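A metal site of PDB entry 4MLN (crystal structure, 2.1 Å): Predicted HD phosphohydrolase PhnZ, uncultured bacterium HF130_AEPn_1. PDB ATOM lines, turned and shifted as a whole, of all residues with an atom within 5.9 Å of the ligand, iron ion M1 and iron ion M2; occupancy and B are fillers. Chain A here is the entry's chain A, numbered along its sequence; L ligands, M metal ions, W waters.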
ATOM      1  N   ILE A  25       7.322  -7.117   1.134  1.00  0.00           N
ATOM      2  CA  ILE A  25       8.201  -6.294   0.290  1.00  0.00           C
ATOM      3  C   ILE A  25       8.353  -6.870  -1.131  1.00  0.00           C
ATOM      4  O   ILE A  25       9.460  -6.978  -1.672  1.00  0.00           O
ATOM      5  CB  ILE A  25       9.590  -5.969   0.935  1.00  0.00           C
ATOM      6  CG1 ILE A  25      10.354  -7.244   1.278  1.00  0.00           C
ATOM      7  CG2 ILE A  25       9.415  -5.075   2.182  1.00  0.00           C
ATOM      8  CD1 ILE A  25      11.721  -6.956   1.879  1.00  0.00           C
ATOM      9  N   GLU A  27       7.864  -9.777  -2.414  1.00  0.00           N
ATOM     10  CA  GLU A  27       8.205 -11.187  -2.636  1.00  0.00           C
ATOM     11  C   GLU A  27       7.002 -12.139  -2.460  1.00  0.00           C
ATOM     12  O   GLU A  27       5.954 -11.737  -1.930  1.00  0.00           O
ATOM     13  CB  GLU A  27       9.375 -11.594  -1.742  1.00  0.00           C
ATOM     14  CG  GLU A  27      10.610 -10.704  -1.870  1.00  0.00           C
ATOM     15  CD  GLU A  27      11.519 -11.069  -3.062  1.00  0.00           C
ATOM     16  OE1 GLU A  27      12.698 -10.629  -3.049  1.00  0.00           O
ATOM     17  OE2 GLU A  27      11.074 -11.783  -3.994  1.00  0.00           O
ATOM     18  N   HIS A  34      11.574 -16.515   3.831  1.00  0.00           N
ATOM     19  CA  HIS A  34      12.730 -16.312   2.971  1.00  0.00           C
ATOM     20  C   HIS A  34      14.051 -16.639   3.691  1.00  0.00           C
ATOM     21  O   HIS A  34      14.887 -17.375   3.182  1.00  0.00           O
ATOM     22  CB  HIS A  34      12.790 -14.880   2.428  1.00  0.00           C
ATOM     23  CG  HIS A  34      14.005 -14.603   1.599  1.00  0.00           C
ATOM     24  ND1 HIS A  34      14.373 -15.400   0.537  1.00  0.00           N
ATOM     25  CD2 HIS A  34      14.956 -13.638   1.688  1.00  0.00           C
ATOM     26  CE1 HIS A  34      15.497 -14.927   0.000  1.00  0.00           C
ATOM     27  NE2 HIS A  34      15.859 -13.856   0.677  1.00  0.00           N
ATOM     28  N   CYS A  38      16.780 -20.050   2.794  1.00  0.00           N
ATOM     29  CA  CYS A  38      18.179 -19.927   2.406  1.00  0.00           C
ATOM     30  C   CYS A  38      19.085 -20.692   3.366  1.00  0.00           C
ATOM     31  O   CYS A  38      20.050 -21.334   2.949  1.00  0.00           O
ATOM     32  CB  CYS A  38      18.584 -18.447   2.348  1.00  0.00           C
ATOM     33  SG  CYS A  38      17.568 -17.473   1.191  1.00  0.00           S
ATOM     34  N   HIS A  58      21.056 -12.967   5.962  1.00  0.00           N
ATOM     35  CA  HIS A  58      21.481 -12.055   4.909  1.00  0.00           C
ATOM     36  C   HIS A  58      20.538 -10.875   4.667  1.00  0.00           C
ATOM     37  O   HIS A  58      20.989  -9.807   4.258  1.00  0.00           O
ATOM     38  CB  HIS A  58      21.768 -12.799   3.590  1.00  0.00           C
ATOM     39  CG  HIS A  58      20.554 -13.057   2.762  1.00  0.00           C
ATOM     40  ND1 HIS A  58      19.782 -14.195   2.906  1.00  0.00           N
ATOM     41  CD2 HIS A  58      19.974 -12.331   1.779  1.00  0.00           C
ATOM     42  CE1 HIS A  58      18.782 -14.155   2.052  1.00  0.00           C
ATOM     43  NE2 HIS A  58      18.875 -13.034   1.351  1.00  0.00           N
ATOM     44  N   ASP A  59      19.234 -11.071   4.893  1.00  0.00           N
ATOM     45  CA  ASP A  59      18.264  -9.976   4.721  1.00  0.00           C
ATOM     46  C   ASP A  59      17.772  -9.343   6.056  1.00  0.00           C
ATOM     47  O   ASP A  59      16.737  -8.662   6.081  1.00  0.00           O
ATOM     48  CB  ASP A  59      17.069 -10.415   3.877  1.00  0.00           C
ATOM     49  CG  ASP A  59      17.345 -10.355   2.391  1.00  0.00           C
ATOM     50  OD1 ASP A  59      18.267  -9.613   1.962  1.00  0.00           O
ATOM     51  OD2 ASP A  59      16.641 -11.029   1.636  1.00  0.00           O
ATOM     52  N   HIS A  62      16.614  -5.455   6.335  1.00  0.00           N
ATOM     53  CA  HIS A  62      15.324  -4.970   5.923  1.00  0.00           C
ATOM     54  C   HIS A  62      14.484  -4.579   7.160  1.00  0.00           C
ATOM     55  O   HIS A  62      13.451  -3.911   7.027  1.00  0.00           O
ATOM     56  CB  HIS A  62      14.582  -6.016   5.084  1.00  0.00           C
ATOM     57  CG  HIS A  62      15.042  -6.113   3.651  1.00  0.00           C
ATOM     58  ND1 HIS A  62      15.292  -5.011   2.861  1.00  0.00           N
ATOM     59  CD2 HIS A  62      15.242  -7.193   2.851  1.00  0.00           C
ATOM     60  CE1 HIS A  62      15.651  -5.402   1.656  1.00  0.00           C
ATOM     61  NE2 HIS A  62      15.622  -6.724   1.608  1.00  0.00           N
ATOM     62  N   MET A  72      13.363   1.736  -1.104  1.00  0.00           N
ATOM     63  CA  MET A  72      13.577   1.187  -2.430  1.00  0.00           C
ATOM     64  C   MET A  72      12.216   1.011  -3.089  1.00  0.00           C
ATOM     65  O   MET A  72      11.894  -0.052  -3.623  1.00  0.00           O
ATOM     66  CB  MET A  72      14.381  -0.120  -2.367  1.00  0.00           C
ATOM     67  CG  MET A  72      15.713   0.070  -1.649  1.00  0.00           C
ATOM     68  SD  MET A  72      17.003  -1.110  -2.047  1.00  0.00           S
ATOM     69  CE  MET A  72      16.495  -2.523  -1.048  1.00  0.00           C
ATOM     70  N   TYR A  75      10.209  -1.854  -1.880  1.00  0.00           N
ATOM     71  CA  TYR A  75      10.843  -3.191  -1.937  1.00  0.00           C
ATOM     72  C   TYR A  75      12.041  -3.417  -0.992  1.00  0.00           C
ATOM     73  O   TYR A  75      12.843  -4.323  -1.210  1.00  0.00           O
ATOM     74  CB  TYR A  75      11.249  -3.513  -3.368  1.00  0.00           C
ATOM     75  CG  TYR A  75      10.098  -3.447  -4.340  1.00  0.00           C
ATOM     76  CD1 TYR A  75       9.261  -4.538  -4.538  1.00  0.00           C
ATOM     77  CD2 TYR A  75       9.849  -2.292  -5.048  1.00  0.00           C
ATOM     78  CE1 TYR A  75       8.211  -4.480  -5.438  1.00  0.00           C
ATOM     79  CE2 TYR A  75       8.805  -2.228  -5.942  1.00  0.00           C
ATOM     80  CZ  TYR A  75       7.987  -3.309  -6.133  1.00  0.00           C
ATOM     81  OH  TYR A  75       6.946  -3.222  -7.033  1.00  0.00           O
ATOM     82  N   HIS A  80      20.184  -2.342   2.967  1.00  0.00           N
ATOM     83  CA  HIS A  80      19.877  -3.433   3.888  1.00  0.00           C
ATOM     84  C   HIS A  80      21.068  -4.382   4.095  1.00  0.00           C
ATOM     85  O   HIS A  80      21.274  -4.877   5.192  1.00  0.00           O
ATOM     86  CB  HIS A  80      18.625  -4.212   3.464  1.00  0.00           C
ATOM     87  CG  HIS A  80      18.846  -5.132   2.286  1.00  0.00           C
ATOM     88  ND1 HIS A  80      19.060  -4.666   1.005  1.00  0.00           N
ATOM     89  CD2 HIS A  80      18.831  -6.485   2.189  1.00  0.00           C
ATOM     90  CE1 HIS A  80      19.188  -5.696   0.185  1.00  0.00           C
ATOM     91  NE2 HIS A  80      19.061  -6.812   0.881  1.00  0.00           N
ATOM     92  N   HIS A 104      26.143  -9.726  -0.581  1.00  0.00           N
ATOM     93  CA  HIS A 104      25.074 -10.413  -1.305  1.00  0.00           C
ATOM     94  C   HIS A 104      24.420  -9.508  -2.341  1.00  0.00           C
ATOM     95  O   HIS A 104      23.840 -10.000  -3.308  1.00  0.00           O
ATOM     96  CB  HIS A 104      24.058 -11.111  -0.360  1.00  0.00           C
ATOM     97  CG  HIS A 104      22.885 -10.259   0.062  1.00  0.00           C
ATOM     98  ND1 HIS A 104      22.913  -9.461   1.193  1.00  0.00           N
ATOM     99  CD2 HIS A 104      21.645 -10.132  -0.458  1.00  0.00           C
ATOM    100  CE1 HIS A 104      21.734  -8.865   1.329  1.00  0.00           C
ATOM    101  NE2 HIS A 104      20.959  -9.252   0.344  1.00  0.00           N
ATOM    102  N   VAL A 105      24.542  -8.190  -2.158  1.00  0.00           N
ATOM    103  CA  VAL A 105      23.980  -7.245  -3.137  1.00  0.00           C
ATOM    104  C   VAL A 105      24.948  -7.016  -4.280  1.00  0.00           C
ATOM    105  O   VAL A 105      24.558  -7.044  -5.450  1.00  0.00           O
ATOM    106  CB  VAL A 105      23.563  -5.883  -2.499  1.00  0.00           C
ATOM    107  CG1 VAL A 105      23.282  -4.842  -3.591  1.00  0.00           C
ATOM    108  CG2 VAL A 105      22.356  -6.077  -1.603  1.00  0.00           C
ATOM    109  N   LYS A 108      24.602  -9.720  -6.710  1.00  0.00           N
ATOM    110  CA  LYS A 108      23.517  -9.515  -7.645  1.00  0.00           C
ATOM    111  C   LYS A 108      23.950  -8.576  -8.770  1.00  0.00           C
ATOM    112  O   LYS A 108      23.656  -8.812  -9.943  1.00  0.00           O
ATOM    113  CB  LYS A 108      22.290  -8.918  -6.942  1.00  0.00           C
ATOM    114  CG  LYS A 108      21.001  -9.104  -7.715  1.00  0.00           C
ATOM    115  CD  LYS A 108      20.056  -7.904  -7.669  1.00  0.00           C
ATOM    116  CE  LYS A 108      19.958  -7.282  -6.299  1.00  0.00           C
ATOM    117  NZ  LYS A 108      18.716  -6.450  -6.165  1.00  0.00           N
ATOM    118  N   SER A 123      13.751 -12.217  -9.063  1.00  0.00           N
ATOM    119  CA  SER A 123      12.372 -11.934  -8.675  1.00  0.00           C
ATOM    120  C   SER A 123      12.059 -10.510  -9.122  1.00  0.00           C
ATOM    121  O   SER A 123      12.973  -9.742  -9.382  1.00  0.00           O
ATOM    122  CB  SER A 123      12.180 -12.084  -7.165  1.00  0.00           C
ATOM    123  OG  SER A 123      12.871 -11.069  -6.456  1.00  0.00           O
ATOM    124  N   ALA A 125      10.876  -8.151  -7.324  1.00  0.00           N
ATOM    125  CA  ALA A 125      11.409  -7.276  -6.285  1.00  0.00           C
ATOM    126  C   ALA A 125      12.912  -7.018  -6.485  1.00  0.00           C
ATOM    127  O   ALA A 125      13.365  -5.879  -6.405  1.00  0.00           O
ATOM    128  CB  ALA A 125      11.118  -7.850  -4.888  1.00  0.00           C
ATOM    129  N   SER A 126      13.685  -8.061  -6.759  1.00  0.00           N
ATOM    130  CA  SER A 126      15.144  -7.916  -6.839  1.00  0.00           C
ATOM    131  C   SER A 126      15.603  -7.047  -8.009  1.00  0.00           C
ATOM    132  O   SER A 126      16.484  -6.191  -7.856  1.00  0.00           O
ATOM    133  CB  SER A 126      15.847  -9.277  -6.860  1.00  0.00           C
ATOM    134  OG  SER A 126      15.838  -9.868  -5.569  1.00  0.00           O
ATOM    135  N   THR A 129      15.102  -3.467  -6.988  1.00  0.00           N
ATOM    136  CA  THR A 129      15.985  -2.900  -5.973  1.00  0.00           C
ATOM    137  C   THR A 129      17.346  -2.586  -6.547  1.00  0.00           C
ATOM    138  O   THR A 129      18.039  -1.698  -6.062  1.00  0.00           O
ATOM    139  CB  THR A 129      16.135  -3.813  -4.744  1.00  0.00           C
ATOM    140  OG1 THR A 129      16.622  -5.082  -5.164  1.00  0.00           O
ATOM    141  CG2 THR A 129      14.798  -3.978  -4.030  1.00  0.00           C
ATOM    142  N   LEU A 130      17.726  -3.295  -7.609  1.00  0.00           N
ATOM    143  CA  LEU A 130      18.989  -3.029  -8.291  1.00  0.00           C
ATOM    144  C   LEU A 130      19.167  -1.519  -8.629  1.00  0.00           C
ATOM    145  O   LEU A 130      20.299  -1.036  -8.698  1.00  0.00           O
ATOM    146  CB  LEU A 130      19.065  -3.854  -9.566  1.00  0.00           C
ATOM    147  CG  LEU A 130      20.415  -3.954 -10.291  1.00  0.00           C
ATOM    148  CD1 LEU A 130      21.511  -4.482  -9.366  1.00  0.00           C
ATOM    149  CD2 LEU A 130      20.300  -4.853 -11.529  1.00  0.00           C
ATOM    150  N   GLN A 133      20.683   0.416  -5.791  1.00  0.00           N
ATOM    151  CA  GLN A 133      21.883  -0.250  -5.290  1.00  0.00           C
ATOM    152  C   GLN A 133      23.124   0.036  -6.133  1.00  0.00           C
ATOM    153  O   GLN A 133      24.218  -0.461  -5.848  1.00  0.00           O
ATOM    154  CB  GLN A 133      21.615  -1.765  -5.157  1.00  0.00           C
ATOM    155  CG  GLN A 133      20.586  -2.066  -4.076  1.00  0.00           C
ATOM    156  CD  GLN A 133      19.982  -3.473  -4.131  1.00  0.00           C
ATOM    157  OE1 GLN A 133      19.941  -4.129  -5.161  1.00  0.00           O
ATOM    158  NE2 GLN A 133      19.477  -3.917  -2.980  1.00  0.00           N
ATOM    159  N   ARG A 158      24.350 -15.826  -2.848  1.00  0.00           N
ATOM    160  CA  ARG A 158      23.380 -15.200  -3.741  1.00  0.00           C
ATOM    161  C   ARG A 158      22.510 -16.251  -4.423  1.00  0.00           C
ATOM    162  O   ARG A 158      21.296 -16.047  -4.630  1.00  0.00           O
ATOM    163  CB  ARG A 158      24.065 -14.269  -4.743  1.00  0.00           C
ATOM    164  CG  ARG A 158      23.125 -13.345  -5.476  1.00  0.00           C
ATOM    165  CD  ARG A 158      22.498 -12.337  -4.547  1.00  0.00           C
ATOM    166  NE  ARG A 158      21.119 -12.019  -4.940  1.00  0.00           N
ATOM    167  CZ  ARG A 158      20.432 -10.966  -4.476  1.00  0.00           C
ATOM    168  NH1 ARG A 158      21.006 -10.120  -3.632  1.00  0.00           N
ATOM    169  NH2 ARG A 158      19.184 -10.770  -4.875  1.00  0.00           N
ATOM    170  N   ASP A 161      19.907 -17.312  -2.210  1.00  0.00           N
ATOM    171  CA  ASP A 161      19.044 -16.159  -2.033  1.00  0.00           C
ATOM    172  C   ASP A 161      17.970 -16.206  -3.122  1.00  0.00           C
ATOM    173  O   ASP A 161      16.781 -16.086  -2.819  1.00  0.00           O
ATOM    174  CB  ASP A 161      19.876 -14.870  -2.129  1.00  0.00           C
ATOM    175  CG  ASP A 161      19.076 -13.612  -1.797  1.00  0.00           C
ATOM    176  OD1 ASP A 161      17.962 -13.695  -1.258  1.00  0.00           O
ATOM    177  OD2 ASP A 161      19.594 -12.511  -2.060  1.00  0.00           O
ATOM    178  N   GLU A 162      18.374 -16.403  -4.373  1.00  0.00           N
ATOM    179  CA  GLU A 162      17.389 -16.438  -5.456  1.00  0.00           C
ATOM    180  C   GLU A 162      16.487 -17.682  -5.363  1.00  0.00           C
ATOM    181  O   GLU A 162      15.364 -17.679  -5.875  1.00  0.00           O
ATOM    182  CB  GLU A 162      18.051 -16.370  -6.837  1.00  0.00           C
ATOM    183  CG  GLU A 162      19.343 -15.570  -6.899  1.00  0.00           C
ATOM    184  CD  GLU A 162      19.159 -14.071  -6.757  1.00  0.00           C
ATOM    185  OE1 GLU A 162      18.015 -13.565  -6.705  1.00  0.00           O
ATOM    186  OE2 GLU A 162      20.201 -13.382  -6.691  1.00  0.00           O
HETATM  187  O1  LIG L   1      17.833  -6.501  -3.026  1.00  0.00           O
HETATM  188  P1  LIG L   1      17.872  -7.976  -2.778  1.00  0.00           P
HETATM  189  O2  LIG L   1      19.209  -8.195  -2.151  1.00  0.00           O
HETATM  190  O3  LIG L   1      17.914  -8.579  -4.144  1.00  0.00           O
HETATM  191  C1  LIG L   1      16.487  -8.632  -1.809  1.00  0.00           C
HETATM  192  O4  LIG L   1      16.742  -8.434  -0.468  1.00  0.00           O
HETATM  193  C2  LIG L   1      15.235  -7.954  -2.260  1.00  0.00           C
HETATM  194  N1  LIG L   1      14.081  -8.537  -1.617  1.00  0.00           N
HETATM  195 FE    FE M   1      18.867  -8.879   0.019  1.00  0.00          FE
HETATM  196 FE    FE M   2      17.358 -12.295   0.144  1.00  0.00          FE
HETATM  197  O   HOH W   1      14.346  -9.674   0.872  1.00  0.00           O
HETATM  198  O   HOH W   2      18.575 -10.803  -0.671  1.00  0.00           O
HETATM  199  O   HOH W   3      15.794 -11.577  -1.127  1.00  0.00           O
HETATM  200  O   HOH W   4      12.093  -6.613  -1.917  1.00  0.00           O
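OE1 of Gln 133 sits close to O of Thr 129 (3.2 Å).
OD2 of Asp 161 lies within salt-bridge range of NH1 of Arg 158 (3.2 Å).
The side-chain hydroxyl (OG) of Ser 123 is in hydrogen-bond range of the backbone NH (N) of Ser 126, 3.1 Å away.
OE2 of Glu 27 lies within hydrogen-bond range of OG of Ser 123 (3.1 Å).
The side-chain hydroxyl of Thr 129 sits at hydrogen-bond distance from the side-chain amino group of Lys 108, at 2.7 Å.
The backbone carbonyl oxygen (O) of His 34 is in hydrogen-bond range of the side-chain sulfur (SG) of Cys 38, 3.3 Å away.
The backbone carbonyl oxygen (O) of His 104 lies within hydrogen-bond range of the guanidinium group (NH1) of Arg 158, at 2.9 Å.
The backbone carbonyl oxygen (O) of Ser 126 is in hydrogen-bond range of the side-chain hydroxyl (OG1) of Thr 129 (2.9 Å).
Iron ion M2 is bound by OD1 of Asp 161 (2.1 Å), NE2 of His 58 (2.1 Å), OD2 of Asp 59 (2.1 Å), water W2 (2.1 Å), water W3 (2.1 Å) and NE2 of His 34 (2.2 Å).
Iron ion M2 has six donor atoms within binding distance.
Water W2 binds iron ion M1, 2.1 Å away.
NE2 of His 104 is bound to iron ion M1 (2.1 Å).
Iron ion M1 is bound by OD1 of Asp 59.
An oxygen (O4) of the ligand is bound to iron ion M1 (2.2 Å).
Iron ion M1 is bound by NE2 of His 80.
Iron ion M1 is bound by O2 of the ligand, at 2.3 Å.
Merely in contact with the ligand: Val 105.
Hydrophobic or aromatic side chains that line the ligand: His 62, His 80, His 104 and Val 105.
The nearest printed residue that does not touch iron ion M1 is His 58 (4.03 Å).
Water W1 bridges N1 of the ligand and NE2 of His 62.
Water W4 lies within hydrogen-bond range of O of Tyr 75 (2.5 Å), O of Ile 25 (2.7 Å) and N1 of the ligand (2.8 Å).
Of the 22 residues printed, 4 come within 4 Å of iron ion M2.
O3 of the ligand is in salt-bridge range of NH2 of Arg 158, 2.6 Å away.
The side-chain hydroxyl (OG1) of Thr 129 lies within hydrogen-bond range of an oxygen (O1) of the ligand (2.8 Å).
The side-chain carboxylate (OE1) of Glu 27 is in salt-bridge range of a nitrogen (N1) of the ligand (2.9 Å).
An oxygen (O3) of the ligand lies within hydrogen-bond range of the side-chain hydroxyl (OG) of Ser 126.
The side-chain amino group (NZ) of Lys 108 lies within salt-bridge range of an oxygen (O3) of the ligand, 3.0 Å away.
A ring nitrogen (NE2) of His 62 sits close to an oxygen (O4) of the ligand (2.9 Å).
An oxygen (O1) of the ligand sits at hydrogen-bond distance from the side-chain amide nitrogen (NE2) of Gln 133, at 3.1 Å.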
